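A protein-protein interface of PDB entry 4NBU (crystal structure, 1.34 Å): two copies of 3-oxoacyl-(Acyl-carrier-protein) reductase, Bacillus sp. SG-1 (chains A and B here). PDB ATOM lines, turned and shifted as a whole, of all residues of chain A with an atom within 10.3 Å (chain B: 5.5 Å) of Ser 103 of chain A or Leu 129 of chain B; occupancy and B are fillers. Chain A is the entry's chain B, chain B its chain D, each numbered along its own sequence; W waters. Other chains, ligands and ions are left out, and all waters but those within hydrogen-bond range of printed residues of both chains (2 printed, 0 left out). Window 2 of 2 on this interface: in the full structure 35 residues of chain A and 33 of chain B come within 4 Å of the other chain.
The backbone NH (N) of Gly 154 of chain A is in hydrogen-bond range of the side-chain carboxylate (OE2) of Glu 175 of chain B, at 2.7 Å.
NE2 of Gln 126 of chain B lies within hydrogen-bond range of O of Met 105 of chain A (2.9 Å).
The side-chain carboxylate of Glu 175 of chain B is in hydrogen-bond range of the backbone NH of Leu 102 of chain A, at 2.9 Å.
O of Leu 102 of chain A is in hydrogen-bond range of NE2 of Gln 126 of chain B (2.7 Å).
The backbone NH of Ser 100 of chain A sits at hydrogen-bond distance from the backbone carbonyl oxygen of Gly 154 of chain A, at 2.9 Å.
The side-chain hydroxyl of Ser 100 of chain A sits at hydrogen-bond distance from the backbone NH of Met 105 of chain A (3.2 Å).
Glu 175 of chain B touches Met 101 of chain A (CG to CE, 3.5 Å).
Leu 102 of chain A touches Thr 125 of chain B (CD2 to CG2, 3.9 Å).
Ser 103 of chain A touches Leu 129 of chain B (CB to CD2, 3.9 Å).
Val 153 of chain A touches Glu 175 of chain B.
Of the printed residues of chain B, Met 101 of chain A touches Glu 175.
Of the printed residues of chain B, Leu 102 of chain A touches Thr 125, Gln 126 and Glu 175.
Ser 103 of chain A touches one residue of chain B.
Cys 124 of chain B touches none of the printed residues of chain A.
Val 128 of chain B touches none of the printed residues of chain A.
Printed residues of chain A within 4 Å of Leu 129 of chain B: Ser 103.
No residue of chain A comes within 4 Å of Pro 130 of chain B.
The nearest residue of chain B that does not touch Ser 103 of chain A is Gln 126 of chain B (4.6 Å).
The nearest printed residue of chain A that does not touch Thr 125 of chain B is Ser 103 of chain A (7.7 Å).
Printed residues of chain A that touch a printed residue of chain B: Met 101, Leu 102, Ser 103, Met 105, Val 153 and Gly 154.
Among the printed residues, 8 pairs touch across the chains.
Among the printed residues, no Asp or Glu carboxylate lies within 4 Å of a Lys or Arg side-chain nitrogen of the other chain.
No position is printed for both chains.
Of the 8 pairs that touch across the chains among the printed residues, none has its exchanged pair printed and touching as well.
Water W2 lies within hydrogen-bond range of OE2 of Glu 175 of chain B (2.6 Å), OG1 of Thr 156 of chain A (2.6 Å), O of Ser 100 of chain A (2.8 Å), N of Gln 155 of chain A (3.3 Å) and N of Leu 102 of chain A (3.4 Å).
Water W1 lies within hydrogen-bond range of OE1 of Glu 175 of chain B, N of Ser 103 of chain A and N of Leu 102 of chain A.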
ATOM      1  N   ASP A  99     -13.682  33.534   2.966  1.00  0.00           N
ATOM      2  CA  ASP A  99     -14.101  32.132   2.946  1.00  0.00           C
ATOM      3  C   ASP A  99     -13.089  31.239   2.241  1.00  0.00           C
ATOM      4  O   ASP A  99     -12.463  31.645   1.254  1.00  0.00           O
ATOM      5  CB  ASP A  99     -15.470  31.977   2.268  1.00  0.00           C
ATOM      6  CG  ASP A  99     -16.616  32.562   3.084  1.00  0.00           C
ATOM      7  OD1 ASP A  99     -16.442  32.879   4.275  1.00  0.00           O
ATOM      8  OD2 ASP A  99     -17.719  32.698   2.515  1.00  0.00           O
ATOM      9  N   SER A 100     -12.960  30.015   2.741  1.00  0.00           N
ATOM     10  CA  SER A 100     -12.109  28.999   2.133  1.00  0.00           C
ATOM     11  C   SER A 100     -12.396  27.669   2.799  1.00  0.00           C
ATOM     12  O   SER A 100     -12.708  27.628   3.980  1.00  0.00           O
ATOM     13  CB  SER A 100     -10.632  29.343   2.329  1.00  0.00           C
ATOM     14  OG  SER A 100      -9.803  28.294   1.844  1.00  0.00           O
ATOM     15  N   MET A 101     -12.294  26.582   2.044  1.00  0.00           N
ATOM     16  CA  MET A 101     -12.335  25.271   2.664  1.00  0.00           C
ATOM     17  C   MET A 101     -11.150  25.181   3.606  1.00  0.00           C
ATOM     18  O   MET A 101     -10.112  25.811   3.362  1.00  0.00           O
ATOM     19  CB  MET A 101     -12.253  24.177   1.602  1.00  0.00           C
ATOM     20  CG  MET A 101     -13.385  24.238   0.596  1.00  0.00           C
ATOM     21  SD  MET A 101     -14.973  23.907   1.386  1.00  0.00           S
ATOM     22  CE  MET A 101     -14.825  22.153   1.698  1.00  0.00           C
ATOM     23  N   LEU A 102     -11.303  24.415   4.682  1.00  0.00           N
ATOM     24  CA  LEU A 102     -10.212  24.228   5.636  1.00  0.00           C
ATOM     25  C   LEU A 102      -8.913  23.823   4.944  1.00  0.00           C
ATOM     26  O   LEU A 102      -7.841  24.337   5.271  1.00  0.00           O
ATOM     27  CB  LEU A 102     -10.588  23.174   6.674  1.00  0.00           C
ATOM     28  CG  LEU A 102      -9.512  22.860   7.712  1.00  0.00           C
ATOM     29  CD1 LEU A 102      -9.167  24.111   8.514  1.00  0.00           C
ATOM     30  CD2 LEU A 102      -9.993  21.732   8.616  1.00  0.00           C
ATOM     31  N   SER A 103      -9.018  22.924   3.968  1.00  0.00           N
ATOM     32  CA  SER A 103      -7.846  22.372   3.298  1.00  0.00           C
ATOM     33  C   SER A 103      -7.017  23.421   2.559  1.00  0.00           C
ATOM     34  O   SER A 103      -5.839  23.186   2.270  1.00  0.00           O
ATOM     35  CB  SER A 103      -8.270  21.272   2.323  1.00  0.00           C
ATOM     36  OG  SER A 103      -9.048  21.807   1.265  1.00  0.00           O
ATOM     37  N   LYS A 104      -7.621  24.569   2.251  1.00  0.00           N
ATOM     38  CA  LYS A 104      -6.949  25.600   1.468  1.00  0.00           C
ATOM     39  C   LYS A 104      -6.798  26.934   2.189  1.00  0.00           C
ATOM     40  O   LYS A 104      -6.187  27.857   1.651  1.00  0.00           O
ATOM     41  CB  LYS A 104      -7.680  25.827   0.136  1.00  0.00           C
ATOM     42  CG  LYS A 104      -7.875  24.557  -0.679  1.00  0.00           C
ATOM     43  CD  LYS A 104      -8.107  24.851  -2.151  1.00  0.00           C
ATOM     44  CE  LYS A 104      -9.470  25.464  -2.400  1.00  0.00           C
ATOM     45  NZ  LYS A 104      -9.771  25.522  -3.861  1.00  0.00           N
ATOM     46  N   MET A 105      -7.340  27.036   3.399  1.00  0.00           N
ATOM     47  CA  MET A 105      -7.402  28.327   4.088  1.00  0.00           C
ATOM     48  C   MET A 105      -6.020  28.783   4.530  1.00  0.00           C
ATOM     49  O   MET A 105      -5.263  28.021   5.127  1.00  0.00           O
ATOM     50  CB  MET A 105      -8.349  28.267   5.294  1.00  0.00           C
ATOM     51  CG  MET A 105      -8.488  29.601   6.029  1.00  0.00           C
ATOM     52  SD  MET A 105      -9.821  29.598   7.246  1.00  0.00           S
ATOM     53  CE  MET A 105     -11.256  29.616   6.181  1.00  0.00           C
ATOM     54  N   THR A 106      -5.677  30.027   4.228  1.00  0.00           N
ATOM     55  CA  THR A 106      -4.377  30.537   4.624  1.00  0.00           C
ATOM     56  C   THR A 106      -4.426  31.116   6.031  1.00  0.00           C
ATOM     57  O   THR A 106      -5.491  31.445   6.549  1.00  0.00           O
ATOM     58  CB  THR A 106      -3.876  31.617   3.661  1.00  0.00           C
ATOM     59  OG1 THR A 106      -4.692  32.785   3.793  1.00  0.00           O
ATOM     60  CG2 THR A 106      -3.945  31.119   2.230  1.00  0.00           C
ATOM     61  N   VAL A 107      -3.260  31.234   6.652  1.00  0.00           N
ATOM     62  CA  VAL A 107      -3.185  31.840   7.973  1.00  0.00           C
ATOM     63  C   VAL A 107      -3.687  33.279   7.920  1.00  0.00           C
ATOM     64  O   VAL A 107      -4.379  33.728   8.828  1.00  0.00           O
ATOM     65  CB  VAL A 107      -1.760  31.765   8.553  1.00  0.00           C
ATOM     66  CG1 VAL A 107      -1.668  32.526   9.867  1.00  0.00           C
ATOM     67  CG2 VAL A 107      -1.377  30.313   8.766  1.00  0.00           C
ATOM     68  N   GLN A 109      -5.994  34.501   5.864  1.00  0.00           N
ATOM     69  CA  GLN A 109      -7.454  34.487   5.802  1.00  0.00           C
ATOM     70  C   GLN A 109      -8.054  34.238   7.180  1.00  0.00           C
ATOM     71  O   GLN A 109      -9.056  34.847   7.557  1.00  0.00           O
ATOM     72  CB  GLN A 109      -7.954  33.414   4.838  1.00  0.00           C
ATOM     73  CG  GLN A 109      -7.838  33.780   3.368  1.00  0.00           C
ATOM     74  CD  GLN A 109      -8.210  32.617   2.469  1.00  0.00           C
ATOM     75  OE1 GLN A 109      -7.832  31.468   2.722  1.00  0.00           O
ATOM     76  NE2 GLN A 109      -8.960  32.904   1.411  1.00  0.00           N
ATOM     77  N   VAL A 153     -20.019  25.271   5.847  1.00  0.00           N
ATOM     78  CA  VAL A 153     -18.924  24.891   4.951  1.00  0.00           C
ATOM     79  C   VAL A 153     -18.229  26.114   4.352  1.00  0.00           C
ATOM     80  O   VAL A 153     -18.882  27.071   3.906  1.00  0.00           O
ATOM     81  CB  VAL A 153     -19.433  23.956   3.834  1.00  0.00           C
ATOM     82  CG1 VAL A 153     -18.402  23.791   2.736  1.00  0.00           C
ATOM     83  CG2 VAL A 153     -19.826  22.600   4.419  1.00  0.00           C
ATOM     84  N   GLY A 154     -16.899  26.092   4.386  1.00  0.00           N
ATOM     85  CA  GLY A 154     -16.095  27.154   3.811  1.00  0.00           C
ATOM     86  C   GLY A 154     -15.867  28.332   4.734  1.00  0.00           C
ATOM     87  O   GLY A 154     -15.277  29.339   4.326  1.00  0.00           O
ATOM     88  N   GLN A 155     -16.326  28.224   5.980  1.00  0.00           N
ATOM     89  CA  GLN A 155     -16.258  29.362   6.892  1.00  0.00           C
ATOM     90  C   GLN A 155     -15.595  29.073   8.237  1.00  0.00           C
ATOM     91  O   GLN A 155     -16.023  29.604   9.257  1.00  0.00           O
ATOM     92  CB  GLN A 155     -17.662  29.929   7.113  1.00  0.00           C
ATOM     93  CG  GLN A 155     -18.321  30.416   5.835  1.00  0.00           C
ATOM     94  CD  GLN A 155     -19.354  31.481   6.103  1.00  0.00           C
ATOM     95  OE1 GLN A 155     -20.459  31.191   6.570  1.00  0.00           O
ATOM     96  NE2 GLN A 155     -18.997  32.732   5.821  1.00  0.00           N
ATOM     97  N   THR A 156     -14.540  28.261   8.237  1.00  0.00           N
ATOM     98  CA  THR A 156     -13.825  27.948   9.474  1.00  0.00           C
ATOM     99  C   THR A 156     -13.530  29.184  10.319  1.00  0.00           C
ATOM    100  O   THR A 156     -13.789  29.208  11.528  1.00  0.00           O
ATOM    101  CB  THR A 156     -12.474  27.258   9.178  1.00  0.00           C
ATOM    102  OG1 THR A 156     -12.707  25.941   8.660  1.00  0.00           O
ATOM    103  CG2 THR A 156     -11.633  27.164  10.440  1.00  0.00           C
ATOM    104  N   ASN A 157     -12.992  30.211   9.668  1.00  0.00           N
ATOM    105  CA  ASN A 157     -12.559  31.419  10.362  1.00  0.00           C
ATOM    106  C   ASN A 157     -13.724  32.272  10.868  1.00  0.00           C
ATOM    107  O   ASN A 157     -13.737  32.717  12.021  1.00  0.00           O
ATOM    108  CB  ASN A 157     -11.613  32.244   9.469  1.00  0.00           C
ATOM    109  CG  ASN A 157     -12.146  32.438   8.039  1.00  0.00           C
ATOM    110  OD1 ASN A 157     -13.205  31.927   7.660  1.00  0.00           O
ATOM    111  ND2 ASN A 157     -11.404  33.204   7.243  1.00  0.00           N
ATOM    112  N   CYS B 124      -3.327  22.661  14.090  1.00  0.00           N
ATOM    113  CA  CYS B 124      -3.174  21.221  14.239  1.00  0.00           C
ATOM    114  C   CYS B 124      -4.119  20.460  13.321  1.00  0.00           C
ATOM    115  O   CYS B 124      -3.736  19.462  12.701  1.00  0.00           O
ATOM    116  CB  CYS B 124      -3.368  20.794  15.694  1.00  0.00           C
ATOM    117  SG  CYS B 124      -2.035  21.325  16.783  1.00  0.00           S
ATOM    118  N   THR B 125      -5.354  20.937  13.227  1.00  0.00           N
ATOM    119  CA  THR B 125      -6.349  20.249  12.420  1.00  0.00           C
ATOM    120  C   THR B 125      -6.006  20.355  10.939  1.00  0.00           C
ATOM    121  O   THR B 125      -6.078  19.369  10.203  1.00  0.00           O
ATOM    122  CB  THR B 125      -7.744  20.789  12.701  1.00  0.00           C
ATOM    123  OG1 THR B 125      -8.002  20.699  14.108  1.00  0.00           O
ATOM    124  CG2 THR B 125      -8.801  19.980  11.948  1.00  0.00           C
ATOM    125  N   GLN B 126      -5.589  21.539  10.506  1.00  0.00           N
ATOM    126  CA  GLN B 126      -5.205  21.702   9.119  1.00  0.00           C
ATOM    127  C   GLN B 126      -4.024  20.799   8.766  1.00  0.00           C
ATOM    128  O   GLN B 126      -3.957  20.250   7.666  1.00  0.00           O
ATOM    129  CB  GLN B 126      -4.860  23.156   8.831  1.00  0.00           C
ATOM    130  CG  GLN B 126      -4.763  23.453   7.360  1.00  0.00           C
ATOM    131  CD  GLN B 126      -4.640  24.929   7.100  1.00  0.00           C
ATOM    132  OE1 GLN B 126      -3.688  25.570   7.548  1.00  0.00           O
ATOM    133  NE2 GLN B 126      -5.616  25.489   6.397  1.00  0.00           N
ATOM    134  N   ALA B 127      -3.101  20.630   9.709  1.00  0.00           N
ATOM    135  CA  ALA B 127      -1.905  19.841   9.451  1.00  0.00           C
ATOM    136  C   ALA B 127      -2.194  18.339   9.350  1.00  0.00           C
ATOM    137  O   ALA B 127      -1.584  17.655   8.540  1.00  0.00           O
ATOM    138  CB  ALA B 127      -0.845  20.114  10.502  1.00  0.00           C
ATOM    139  N   VAL B 128      -3.112  17.827  10.167  1.00  0.00           N
ATOM    140  CA  VAL B 128      -3.434  16.401  10.108  1.00  0.00           C
ATOM    141  C   VAL B 128      -4.388  16.061   8.965  1.00  0.00           C
ATOM    142  O   VAL B 128      -4.401  14.934   8.481  1.00  0.00           O
ATOM    143  CB  VAL B 128      -4.010  15.852  11.441  1.00  0.00           C
ATOM    144  CG1 VAL B 128      -3.078  16.160  12.605  1.00  0.00           C
ATOM    145  CG2 VAL B 128      -5.440  16.337  11.689  1.00  0.00           C
ATOM    146  N   LEU B 129      -5.170  17.044   8.530  1.00  0.00           N
ATOM    147  CA  LEU B 129      -6.219  16.809   7.536  1.00  0.00           C
ATOM    148  C   LEU B 129      -5.800  16.026   6.279  1.00  0.00           C
ATOM    149  O   LEU B 129      -6.480  15.072   5.906  1.00  0.00           O
ATOM    150  CB  LEU B 129      -6.909  18.126   7.160  1.00  0.00           C
ATOM    151  CG  LEU B 129      -7.963  18.024   6.058  1.00  0.00           C
ATOM    152  CD1 LEU B 129      -9.120  17.117   6.486  1.00  0.00           C
ATOM    153  CD2 LEU B 129      -8.468  19.414   5.702  1.00  0.00           C
ATOM    154  N   PRO B 130      -4.688  16.412   5.617  1.00  0.00           N
ATOM    155  CA  PRO B 130      -4.333  15.677   4.399  1.00  0.00           C
ATOM    156  C   PRO B 130      -4.148  14.180   4.638  1.00  0.00           C
ATOM    157  O   PRO B 130      -4.469  13.371   3.769  1.00  0.00           O
ATOM    158  CB  PRO B 130      -2.979  16.277   4.006  1.00  0.00           C
ATOM    159  CG  PRO B 130      -2.943  17.589   4.618  1.00  0.00           C
ATOM    160  CD  PRO B 130      -3.786  17.556   5.853  1.00  0.00           C
ATOM    161  N   TYR B 131      -3.639  13.825   5.811  1.00  0.00           N
ATOM    162  CA  TYR B 131      -3.407  12.426   6.138  1.00  0.00           C
ATOM    163  C   TYR B 131      -4.727  11.698   6.326  1.00  0.00           C
ATOM    164  O   TYR B 131      -4.923  10.603   5.796  1.00  0.00           O
ATOM    165  CB  TYR B 131      -2.528  12.318   7.385  1.00  0.00           C
ATOM    166  CG  TYR B 131      -1.153  12.893   7.152  1.00  0.00           C
ATOM    167  CD1 TYR B 131      -0.201  12.178   6.439  1.00  0.00           C
ATOM    168  CD2 TYR B 131      -0.816  14.163   7.609  1.00  0.00           C
ATOM    169  CE1 TYR B 131       1.054  12.701   6.200  1.00  0.00           C
ATOM    170  CE2 TYR B 131       0.442  14.691   7.376  1.00  0.00           C
ATOM    171  CZ  TYR B 131       1.371  13.956   6.673  1.00  0.00           C
ATOM    172  OH  TYR B 131       2.626  14.475   6.440  1.00  0.00           O
ATOM    173  N   MET B 132      -5.640  12.314   7.063  1.00  0.00           N
ATOM    174  CA  MET B 132      -6.941  11.704   7.281  1.00  0.00           C
ATOM    175  C   MET B 132      -7.745  11.619   5.991  1.00  0.00           C
ATOM    176  O   MET B 132      -8.418  10.619   5.741  1.00  0.00           O
ATOM    177  CB  MET B 132      -7.711  12.471   8.345  1.00  0.00           C
ATOM    178  CG  MET B 132      -7.112  12.351   9.729  1.00  0.00           C
ATOM    179  SD  MET B 132      -8.112  13.227  10.941  1.00  0.00           S
ATOM    180  CE  MET B 132      -7.253  12.806  12.458  1.00  0.00           C
ATOM    181  N   ALA B 133      -7.668  12.658   5.163  1.00  0.00           N
ATOM    182  CA  ALA B 133      -8.378  12.659   3.886  1.00  0.00           C
ATOM    183  C   ALA B 133      -7.871  11.562   2.959  1.00  0.00           C
ATOM    184  O   ALA B 133      -8.654  10.912   2.264  1.00  0.00           O
ATOM    185  CB  ALA B 133      -8.270  14.026   3.216  1.00  0.00           C
ATOM    186  N   GLU B 134      -6.559  11.345   2.955  1.00  0.00           N
ATOM    187  CA  GLU B 134      -5.977  10.327   2.093  1.00  0.00           C
ATOM    188  C   GLU B 134      -6.410   8.925   2.519  1.00  0.00           C
ATOM    189  O   GLU B 134      -6.594   8.044   1.676  1.00  0.00           O
ATOM    190  CB  GLU B 134      -4.449  10.447   2.065  1.00  0.00           C
ATOM    191  CG  GLU B 134      -3.769   9.589   1.001  1.00  0.00           C
ATOM    192  CD  GLU B 134      -3.471   8.183   1.483  1.00  0.00           C
ATOM    193  OE1 GLU B 134      -3.100   8.027   2.667  1.00  0.00           O
ATOM    194  OE2 GLU B 134      -3.611   7.234   0.680  1.00  0.00           O
ATOM    195  N   GLU B 175     -17.916  19.981   6.754  1.00  0.00           N
ATOM    196  CA  GLU B 175     -16.977  19.954   5.632  1.00  0.00           C
ATOM    197  C   GLU B 175     -16.315  18.601   5.409  1.00  0.00           C
ATOM    198  O   GLU B 175     -16.058  18.204   4.273  1.00  0.00           O
ATOM    199  CB  GLU B 175     -15.867  20.975   5.868  1.00  0.00           C
ATOM    200  CG  GLU B 175     -16.004  22.218   5.044  1.00  0.00           C
ATOM    201  CD  GLU B 175     -14.856  23.193   5.235  1.00  0.00           C
ATOM    202  OE1 GLU B 175     -13.669  22.808   5.089  1.00  0.00           O
ATOM    203  OE2 GLU B 175     -15.158  24.351   5.522  1.00  0.00           O
ATOM    204  N   LEU B 176     -16.023  17.911   6.503  1.00  0.00           N
ATOM    205  CA  LEU B 176     -15.146  16.738   6.455  1.00  0.00           C
ATOM    206  C   LEU B 176     -15.894  15.417   6.488  1.00  0.00           C
ATOM    207  O   LEU B 176     -15.289  14.357   6.349  1.00  0.00           O
ATOM    208  CB  LEU B 176     -14.129  16.782   7.599  1.00  0.00           C
ATOM    209  CG  LEU B 176     -13.305  18.067   7.677  1.00  0.00           C
ATOM    210  CD1 LEU B 176     -12.279  17.990   8.794  1.00  0.00           C
ATOM    211  CD2 LEU B 176     -12.628  18.343   6.342  1.00  0.00           C
ATOM    212  N   ILE B 181     -14.455  11.530   8.069  1.00  0.00           N
ATOM    213  CA  ILE B 181     -13.915  12.079   9.304  1.00  0.00           C
ATOM    214  C   ILE B 181     -15.037  12.561  10.225  1.00  0.00           C
ATOM    215  O   ILE B 181     -15.944  13.265   9.782  1.00  0.00           O
ATOM    216  CB  ILE B 181     -12.951  13.240   8.986  1.00  0.00           C
ATOM    217  CG1 ILE B 181     -11.793  12.741   8.112  1.00  0.00           C
ATOM    218  CG2 ILE B 181     -12.443  13.901  10.268  1.00  0.00           C
ATOM    219  CD1 ILE B 181     -10.934  13.850   7.549  1.00  0.00           C
HETATM  220  O   HOH W   1     -11.545  21.312   3.794  1.00  0.00           O
HETATM  221  O   HOH W   2     -13.650  26.307   6.211  1.00  0.00           O
